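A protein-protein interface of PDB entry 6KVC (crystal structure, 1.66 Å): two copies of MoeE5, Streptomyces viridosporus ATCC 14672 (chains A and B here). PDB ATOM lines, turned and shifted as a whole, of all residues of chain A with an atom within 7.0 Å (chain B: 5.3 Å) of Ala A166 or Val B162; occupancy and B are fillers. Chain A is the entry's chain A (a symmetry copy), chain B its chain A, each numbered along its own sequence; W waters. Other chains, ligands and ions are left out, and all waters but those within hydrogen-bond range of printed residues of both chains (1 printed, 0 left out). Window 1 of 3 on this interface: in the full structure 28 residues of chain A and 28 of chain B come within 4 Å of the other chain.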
ATOM      1  N   LEU A 110      -5.406 -21.170 -14.808  1.00  0.00           N
ATOM      2  CA  LEU A 110      -5.283 -21.917 -13.553  1.00  0.00           C
ATOM      3  C   LEU A 110      -3.863 -22.422 -13.358  1.00  0.00           C
ATOM      4  O   LEU A 110      -3.311 -22.378 -12.252  1.00  0.00           O
ATOM      5  CB  LEU A 110      -6.231 -23.112 -13.572  1.00  0.00           C
ATOM      6  CG  LEU A 110      -7.663 -22.891 -13.223  1.00  0.00           C
ATOM      7  CD1 LEU A 110      -8.349 -24.282 -13.305  1.00  0.00           C
ATOM      8  CD2 LEU A 110      -7.761 -22.305 -11.774  1.00  0.00           C
ATOM      9  N   ASN A 113      -1.461 -19.205 -12.837  1.00  0.00           N
ATOM     10  CA  ASN A 113      -1.764 -18.245 -11.780  1.00  0.00           C
ATOM     11  C   ASN A 113      -2.022 -18.924 -10.452  1.00  0.00           C
ATOM     12  O   ASN A 113      -1.798 -18.295  -9.414  1.00  0.00           O
ATOM     13  CB  ASN A 113      -3.003 -17.387 -12.166  1.00  0.00           C
ATOM     14  CG  ASN A 113      -2.722 -16.476 -13.348  1.00  0.00           C
ATOM     15  OD1 ASN A 113      -1.609 -16.511 -13.900  1.00  0.00           O
ATOM     16  ND2 ASN A 113      -3.697 -15.619 -13.712  1.00  0.00           N
ATOM     17  N   VAL A 114      -2.475 -20.183 -10.442  1.00  0.00           N
ATOM     18  CA  VAL A 114      -2.846 -20.856  -9.191  1.00  0.00           C
ATOM     19  C   VAL A 114      -1.924 -22.035  -8.901  1.00  0.00           C
ATOM     20  O   VAL A 114      -1.289 -22.099  -7.841  1.00  0.00           O
ATOM     21  CB  VAL A 114      -4.334 -21.291  -9.201  1.00  0.00           C
ATOM     22  CG1 VAL A 114      -4.743 -21.741  -7.830  1.00  0.00           C
ATOM     23  CG2 VAL A 114      -5.234 -20.085  -9.647  1.00  0.00           C
ATOM     24  N   THR A 117       1.599 -20.846  -8.325  1.00  0.00           N
ATOM     25  CA  THR A 117       1.684 -20.206  -7.013  1.00  0.00           C
ATOM     26  C   THR A 117       1.787 -21.232  -5.893  1.00  0.00           C
ATOM     27  O   THR A 117       2.599 -21.066  -4.968  1.00  0.00           O
ATOM     28  CB  THR A 117       0.467 -19.290  -6.811  1.00  0.00           C
ATOM     29  OG1 THR A 117       0.507 -18.246  -7.793  1.00  0.00           O
ATOM     30  CG2 THR A 117       0.544 -18.588  -5.435  1.00  0.00           C
ATOM     31  N   VAL A 140      -9.800  -8.573  -7.768  1.00  0.00           N
ATOM     32  CA  VAL A 140     -10.523  -9.387  -6.792  1.00  0.00           C
ATOM     33  C   VAL A 140     -11.781  -8.693  -6.313  1.00  0.00           C
ATOM     34  O   VAL A 140     -12.678  -9.353  -5.813  1.00  0.00           O
ATOM     35  CB  VAL A 140      -9.641  -9.785  -5.576  1.00  0.00           C
ATOM     36  CG1 VAL A 140      -8.322 -10.487  -6.028  1.00  0.00           C
ATOM     37  CG2 VAL A 140      -9.349  -8.551  -4.657  1.00  0.00           C
ATOM     38  N   TYR A 160     -10.059 -14.494 -14.453  1.00  0.00           N
ATOM     39  CA  TYR A 160      -8.752 -13.975 -14.063  1.00  0.00           C
ATOM     40  C   TYR A 160      -8.764 -13.485 -12.618  1.00  0.00           C
ATOM     41  O   TYR A 160      -7.880 -13.837 -11.831  1.00  0.00           O
ATOM     42  CB  TYR A 160      -8.339 -12.821 -14.993  1.00  0.00           C
ATOM     43  CG  TYR A 160      -7.178 -12.030 -14.470  1.00  0.00           C
ATOM     44  CD1 TYR A 160      -5.886 -12.562 -14.439  1.00  0.00           C
ATOM     45  CD2 TYR A 160      -7.361 -10.721 -14.019  1.00  0.00           C
ATOM     46  CE1 TYR A 160      -4.798 -11.834 -13.928  1.00  0.00           C
ATOM     47  CE2 TYR A 160      -6.269  -9.955 -13.516  1.00  0.00           C
ATOM     48  CZ  TYR A 160      -5.016 -10.518 -13.484  1.00  0.00           C
ATOM     49  OH  TYR A 160      -3.976  -9.761 -13.042  1.00  0.00           O
ATOM     50  N   GLY A 161      -9.746 -12.644 -12.274  1.00  0.00           N
ATOM     51  CA  GLY A 161      -9.838 -12.174 -10.906  1.00  0.00           C
ATOM     52  C   GLY A 161      -9.964 -13.323  -9.910  1.00  0.00           C
ATOM     53  O   GLY A 161      -9.422 -13.246  -8.802  1.00  0.00           O
ATOM     54  N   VAL A 162     -10.736 -14.374 -10.269  1.00  0.00           N
ATOM     55  CA  VAL A 162     -10.789 -15.562  -9.406  1.00  0.00           C
ATOM     56  C   VAL A 162      -9.404 -16.161  -9.218  1.00  0.00           C
ATOM     57  O   VAL A 162      -9.018 -16.502  -8.089  1.00  0.00           O
ATOM     58  CB  VAL A 162     -11.750 -16.617  -9.956  1.00  0.00           C
ATOM     59  CG1 VAL A 162     -11.728 -17.867  -9.010  1.00  0.00           C
ATOM     60  CG2 VAL A 162     -13.169 -15.996 -10.000  1.00  0.00           C
ATOM     61  N   THR A 163      -8.622 -16.267 -10.294  1.00  0.00           N
ATOM     62  CA  THR A 163      -7.286 -16.854 -10.115  1.00  0.00           C
ATOM     63  C   THR A 163      -6.362 -15.988  -9.264  1.00  0.00           C
ATOM     64  O   THR A 163      -5.540 -16.534  -8.517  1.00  0.00           O
ATOM     65  CB  THR A 163      -6.591 -17.170 -11.465  1.00  0.00           C
ATOM     66  OG1 THR A 163      -6.237 -15.970 -12.200  1.00  0.00           O
ATOM     67  CG2 THR A 163      -7.477 -18.095 -12.323  1.00  0.00           C
ATOM     68  N   LYS A 164      -6.492 -14.649  -9.333  1.00  0.00           N
ATOM     69  CA  LYS A 164      -5.619 -13.815  -8.508  1.00  0.00           C
ATOM     70  C   LYS A 164      -6.045 -13.899  -7.045  1.00  0.00           C
ATOM     71  O   LYS A 164      -5.195 -13.951  -6.147  1.00  0.00           O
ATOM     72  CB  LYS A 164      -5.669 -12.348  -8.996  1.00  0.00           C
ATOM     73  CG  LYS A 164      -5.076 -12.164 -10.445  1.00  0.00           C
ATOM     74  CD  LYS A 164      -3.622 -12.730 -10.580  1.00  0.00           C
ATOM     75  CE  LYS A 164      -2.619 -12.010  -9.676  1.00  0.00           C
ATOM     76  NZ  LYS A 164      -1.243 -12.455 -10.007  1.00  0.00           N
ATOM     77  N   LEU A 165      -7.364 -13.950  -6.793  1.00  0.00           N
ATOM     78  CA  LEU A 165      -7.845 -14.172  -5.418  1.00  0.00           C
ATOM     79  C   LEU A 165      -7.355 -15.517  -4.880  1.00  0.00           C
ATOM     80  O   LEU A 165      -6.864 -15.608  -3.751  1.00  0.00           O
ATOM     81  CB  LEU A 165      -9.367 -14.114  -5.401  1.00  0.00           C
ATOM     82  CG  LEU A 165      -9.994 -14.375  -4.025  1.00  0.00           C
ATOM     83  CD1 LEU A 165      -9.621 -13.284  -2.988  1.00  0.00           C
ATOM     84  CD2 LEU A 165     -11.508 -14.458  -4.166  1.00  0.00           C
ATOM     85  N   ALA A 166      -7.397 -16.557  -5.721  1.00  0.00           N
ATOM     86  CA  ALA A 166      -6.914 -17.875  -5.279  1.00  0.00           C
ATOM     87  C   ALA A 166      -5.423 -17.859  -4.970  1.00  0.00           C
ATOM     88  O   ALA A 166      -4.992 -18.423  -3.959  1.00  0.00           O
ATOM     89  CB  ALA A 166      -7.258 -18.930  -6.329  1.00  0.00           C
ATOM     90  N   ALA A 167      -4.628 -17.170  -5.804  1.00  0.00           N
ATOM     91  CA  ALA A 167      -3.197 -17.080  -5.580  1.00  0.00           C
ATOM     92  C   ALA A 167      -2.910 -16.369  -4.263  1.00  0.00           C
ATOM     93  O   ALA A 167      -2.100 -16.830  -3.453  1.00  0.00           O
ATOM     94  CB  ALA A 167      -2.554 -16.353  -6.765  1.00  0.00           C
ATOM     95  N   GLU A 168      -3.589 -15.250  -4.015  1.00  0.00           N
ATOM     96  CA  GLU A 168      -3.314 -14.531  -2.772  1.00  0.00           C
ATOM     97  C   GLU A 168      -3.825 -15.280  -1.566  1.00  0.00           C
ATOM     98  O   GLU A 168      -3.092 -15.387  -0.571  1.00  0.00           O
ATOM     99  CB  GLU A 168      -3.836 -13.093  -2.791  1.00  0.00           C
ATOM    100  CG  GLU A 168      -5.172 -12.855  -3.067  1.00  0.00           C
ATOM    101  CD  GLU A 168      -5.664 -11.543  -2.328  1.00  0.00           C
ATOM    102  OE1 GLU A 168      -5.353 -10.415  -2.757  1.00  0.00           O
ATOM    103  OE2 GLU A 168      -6.356 -11.667  -1.314  1.00  0.00           O
ATOM    104  N   ARG A 169      -4.983 -15.897  -1.644  1.00  0.00           N
ATOM    105  CA  ARG A 169      -5.399 -16.719  -0.492  1.00  0.00           C
ATOM    106  C   ARG A 169      -4.472 -17.922  -0.272  1.00  0.00           C
ATOM    107  O   ARG A 169      -4.225 -18.313   0.880  1.00  0.00           O
ATOM    108  CB  ARG A 169      -6.823 -17.196  -0.679  1.00  0.00           C
ATOM    109  CG  ARG A 169      -7.861 -16.046  -0.760  1.00  0.00           C
ATOM    110  CD  ARG A 169      -8.073 -15.270   0.581  1.00  0.00           C
ATOM    111  NE  ARG A 169      -7.453 -13.931   0.529  1.00  0.00           N
ATOM    112  CZ  ARG A 169      -7.433 -13.079   1.567  1.00  0.00           C
ATOM    113  NH1 ARG A 169      -6.863 -11.871   1.441  1.00  0.00           N
ATOM    114  NH2 ARG A 169      -7.979 -13.424   2.740  1.00  0.00           N
ATOM    115  N   LEU A 170      -4.007 -18.569  -1.348  1.00  0.00           N
ATOM    116  CA  LEU A 170      -3.026 -19.647  -1.173  1.00  0.00           C
ATOM    117  C   LEU A 170      -1.807 -19.165  -0.418  1.00  0.00           C
ATOM    118  O   LEU A 170      -1.327 -19.820   0.513  1.00  0.00           O
ATOM    119  CB  LEU A 170      -2.582 -20.164  -2.530  1.00  0.00           C
ATOM    120  CG  LEU A 170      -3.437 -21.230  -3.114  1.00  0.00           C
ATOM    121  CD1 LEU A 170      -2.910 -21.397  -4.583  1.00  0.00           C
ATOM    122  CD2 LEU A 170      -3.266 -22.504  -2.220  1.00  0.00           C
ATOM    123  N   ALA A 171      -1.258 -18.019  -0.842  1.00  0.00           N
ATOM    124  CA  ALA A 171      -0.066 -17.480  -0.210  1.00  0.00           C
ATOM    125  C   ALA A 171      -0.289 -17.285   1.278  1.00  0.00           C
ATOM    126  O   ALA A 171       0.545 -17.695   2.086  1.00  0.00           O
ATOM    127  CB  ALA A 171       0.322 -16.166  -0.875  1.00  0.00           C
ATOM    128  N   LEU A 172      -1.444 -16.708   1.650  1.00  0.00           N
ATOM    129  CA  LEU A 172      -1.757 -16.508   3.063  1.00  0.00           C
ATOM    130  C   LEU A 172      -1.906 -17.838   3.804  1.00  0.00           C
ATOM    131  O   LEU A 172      -1.490 -17.950   4.984  1.00  0.00           O
ATOM    132  CB  LEU A 172      -3.019 -15.653   3.176  1.00  0.00           C
ATOM    133  CG  LEU A 172      -2.768 -14.212   2.669  1.00  0.00           C
ATOM    134  CD1 LEU A 172      -4.061 -13.504   2.603  1.00  0.00           C
ATOM    135  CD2 LEU A 172      -1.777 -13.423   3.569  1.00  0.00           C
ATOM    136  N   ALA A 173      -2.497 -18.854   3.148  1.00  0.00           N
ATOM    137  CA  ALA A 173      -2.639 -20.147   3.823  1.00  0.00           C
ATOM    138  C   ALA A 173      -1.279 -20.760   4.110  1.00  0.00           C
ATOM    139  O   ALA A 173      -1.084 -21.387   5.157  1.00  0.00           O
ATOM    140  CB  ALA A 173      -3.474 -21.099   2.971  1.00  0.00           C
ATOM    141  N   PRO B 156      -9.161 -19.047   3.822  1.00  0.00           N
ATOM    142  CA  PRO B 156      -8.954 -20.512   3.958  1.00  0.00           C
ATOM    143  C   PRO B 156      -7.554 -20.860   4.419  1.00  0.00           C
ATOM    144  O   PRO B 156      -6.561 -20.209   4.077  1.00  0.00           O
ATOM    145  CB  PRO B 156      -9.202 -21.065   2.538  1.00  0.00           C
ATOM    146  CG  PRO B 156      -9.167 -19.827   1.621  1.00  0.00           C
ATOM    147  CD  PRO B 156      -9.632 -18.661   2.482  1.00  0.00           C
ATOM    148  N   SER B 158      -6.410 -24.132   4.050  1.00  0.00           N
ATOM    149  CA  SER B 158      -5.947 -25.281   3.275  1.00  0.00           C
ATOM    150  C   SER B 158      -6.109 -24.988   1.798  1.00  0.00           C
ATOM    151  O   SER B 158      -6.962 -24.182   1.391  1.00  0.00           O
ATOM    152  CB  SER B 158      -6.726 -26.571   3.615  1.00  0.00           C
ATOM    153  OG  SER B 158      -8.112 -26.364   3.350  1.00  0.00           O
ATOM    154  N   PRO B 159      -5.354 -25.669   0.947  1.00  0.00           N
ATOM    155  CA  PRO B 159      -5.612 -25.522  -0.504  1.00  0.00           C
ATOM    156  C   PRO B 159      -6.999 -25.974  -0.900  1.00  0.00           C
ATOM    157  O   PRO B 159      -7.585 -25.372  -1.806  1.00  0.00           O
ATOM    158  CB  PRO B 159      -4.508 -26.380  -1.154  1.00  0.00           C
ATOM    159  CG  PRO B 159      -3.389 -26.327  -0.097  1.00  0.00           C
ATOM    160  CD  PRO B 159      -4.120 -26.424   1.232  1.00  0.00           C
ATOM    161  N   TYR B 160      -7.574 -26.969  -0.212  1.00  0.00           N
ATOM    162  CA  TYR B 160      -8.960 -27.349  -0.466  1.00  0.00           C
ATOM    163  C   TYR B 160      -9.899 -26.162  -0.276  1.00  0.00           C
ATOM    164  O   TYR B 160     -10.740 -25.885  -1.136  1.00  0.00           O
ATOM    165  CB  TYR B 160      -9.380 -28.491   0.475  1.00  0.00           C
ATOM    166  CG  TYR B 160     -10.861 -28.716   0.504  1.00  0.00           C
ATOM    167  CD1 TYR B 160     -11.538 -29.271  -0.586  1.00  0.00           C
ATOM    168  CD2 TYR B 160     -11.603 -28.396   1.643  1.00  0.00           C
ATOM    169  CE1 TYR B 160     -12.929 -29.463  -0.575  1.00  0.00           C
ATOM    170  CE2 TYR B 160     -13.012 -28.601   1.687  1.00  0.00           C
ATOM    171  CZ  TYR B 160     -13.646 -29.131   0.589  1.00  0.00           C
ATOM    172  OH  TYR B 160     -14.985 -29.361   0.659  1.00  0.00           O
ATOM    173  N   GLY B 161      -9.782 -25.477   0.868  1.00  0.00           N
ATOM    174  CA  GLY B 161     -10.617 -24.313   1.093  1.00  0.00           C
ATOM    175  C   GLY B 161     -10.437 -23.258   0.005  1.00  0.00           C
ATOM    176  O   GLY B 161     -11.404 -22.587  -0.374  1.00  0.00           O
ATOM    177  N   VAL B 162      -9.185 -23.055  -0.463  1.00  0.00           N
ATOM    178  CA  VAL B 162      -8.974 -22.146  -1.597  1.00  0.00           C
ATOM    179  C   VAL B 162      -9.759 -22.604  -2.816  1.00  0.00           C
ATOM    180  O   VAL B 162     -10.415 -21.787  -3.481  1.00  0.00           O
ATOM    181  CB  VAL B 162      -7.490 -22.012  -1.945  1.00  0.00           C
ATOM    182  CG1 VAL B 162      -7.343 -21.062  -3.183  1.00  0.00           C
ATOM    183  CG2 VAL B 162      -6.762 -21.416  -0.715  1.00  0.00           C
ATOM    184  N   THR B 163      -9.743 -23.905  -3.112  1.00  0.00           N
ATOM    185  CA  THR B 163     -10.496 -24.349  -4.295  1.00  0.00           C
ATOM    186  C   THR B 163     -12.004 -24.183  -4.140  1.00  0.00           C
ATOM    187  O   THR B 163     -12.685 -23.886  -5.131  1.00  0.00           O
ATOM    188  CB  THR B 163     -10.179 -25.816  -4.684  1.00  0.00           C
ATOM    189  OG1 THR B 163     -10.674 -26.767  -3.706  1.00  0.00           O
ATOM    190  CG2 THR B 163      -8.664 -25.999  -4.906  1.00  0.00           C
ATOM    191  N   LYS B 164     -12.546 -24.337  -2.917  1.00  0.00           N
ATOM    192  CA  LYS B 164     -13.989 -24.165  -2.760  1.00  0.00           C
ATOM    193  C   LYS B 164     -14.354 -22.687  -2.864  1.00  0.00           C
ATOM    194  O   LYS B 164     -15.375 -22.334  -3.468  1.00  0.00           O
ATOM    195  CB  LYS B 164     -14.449 -24.734  -1.397  1.00  0.00           C
ATOM    196  CG  LYS B 164     -14.261 -26.296  -1.291  1.00  0.00           C
ATOM    197  CD  LYS B 164     -14.955 -27.069  -2.462  1.00  0.00           C
ATOM    198  CE  LYS B 164     -16.473 -26.880  -2.480  1.00  0.00           C
ATOM    199  NZ  LYS B 164     -17.077 -27.798  -3.478  1.00  0.00           N
ATOM    200  N   LEU B 165     -13.506 -21.805  -2.307  1.00  0.00           N
ATOM    201  CA  LEU B 165     -13.719 -20.359  -2.487  1.00  0.00           C
ATOM    202  C   LEU B 165     -13.661 -19.981  -3.969  1.00  0.00           C
ATOM    203  O   LEU B 165     -14.517 -19.246  -4.470  1.00  0.00           O
ATOM    204  CB  LEU B 165     -12.664 -19.592  -1.700  1.00  0.00           C
ATOM    205  CG  LEU B 165     -12.755 -18.066  -1.844  1.00  0.00           C
ATOM    206  CD1 LEU B 165     -14.071 -17.494  -1.258  1.00  0.00           C
ATOM    207  CD2 LEU B 165     -11.559 -17.422  -1.156  1.00  0.00           C
ATOM    208  N   ALA B 166     -12.702 -20.557  -4.704  1.00  0.00           N
ATOM    209  CA  ALA B 166     -12.606 -20.261  -6.142  1.00  0.00           C
ATOM    210  C   ALA B 166     -13.833 -20.742  -6.904  1.00  0.00           C
ATOM    211  O   ALA B 166     -14.353 -20.022  -7.763  1.00  0.00           O
ATOM    212  CB  ALA B 166     -11.322 -20.864  -6.708  1.00  0.00           C
ATOM    213  N   ALA B 167     -14.341 -21.937  -6.564  1.00  0.00           N
ATOM    214  CA  ALA B 167     -15.521 -22.470  -7.218  1.00  0.00           C
ATOM    215  C   ALA B 167     -16.723 -21.568  -6.963  1.00  0.00           C
ATOM    216  O   ALA B 167     -17.468 -21.222  -7.885  1.00  0.00           O
ATOM    217  CB  ALA B 167     -15.768 -23.895  -6.714  1.00  0.00           C
HETATM  218  O   HOH W   1      -6.381 -17.745   2.758  1.00  0.00           O
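The side-chain carboxylate (OE2) of Glu A168 is in salt-bridge range of the guanidinium group (NH1) of Arg A169.
Among the printed residues, merely in contact across the chains: Ala A173 with Pro B156 (3.4 Å), Val A162 with Ala B166 (3.6 Å), Ala A166 with Val B162 (3.6 Å), Leu A170 with Val B162 (3.9 Å) and Arg A169 with Leu B165 (3.97 Å).
Printed residues of chain B within 4 Å of Val A162: Ala B166.
Leu A165 touches none of the printed residues of chain B.
Of chain B, only Val B162 comes within 4 Å of Ala A166.
Of the printed residues of chain B, Ala A173 touches Pro B156.
Of the printed residues of chain A, Pro B156 touches Ala A173 (3.4 Å).
No residue of chain A comes within 4 Å of Gly B161.
Of chain A, only Ala A166 (3.6 Å) and Leu A170 (3.9 Å) come within 4 Å of Val B162.
Of the printed residues of chain A, Leu B165 touches Arg A169 (3.97 Å).
The nearest residue of chain B that does not touch Ala A166 is Ala B166 (4.5 Å).
The nearest residue of chain A that does not touch Val B162 is Arg A169 (4.2 Å).
The nearest printed residue of chain A that does not touch Leu B165 is Leu A165 (4.2 Å).
Along chain B the printed residues that touch a printed residue of chain A span positions 156 to 166.
Hydrophobic or aromatic side chains of chain A that line the printed part of chain B: Val A162, Ala A166, Leu A170 and Ala A173.
Among the printed residues, 5 pairs touch across the chains.
Val A162 touches Ala B166, and with the chains exchanged Ala A166 touches Val B162.
Positions printed for both chains: 160, 161, 162, 163, 164, 165, 166 and 167.
Of the 5 pairs that touch across the chains among the printed residues, 2 have their exchanged pair printed and touching as well.
Water W1 bridges the backbone carbonyl oxygen of Pro B156 (2.8 Å) and the backbone carbonyl oxygen of Arg A169 (2.9 Å).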
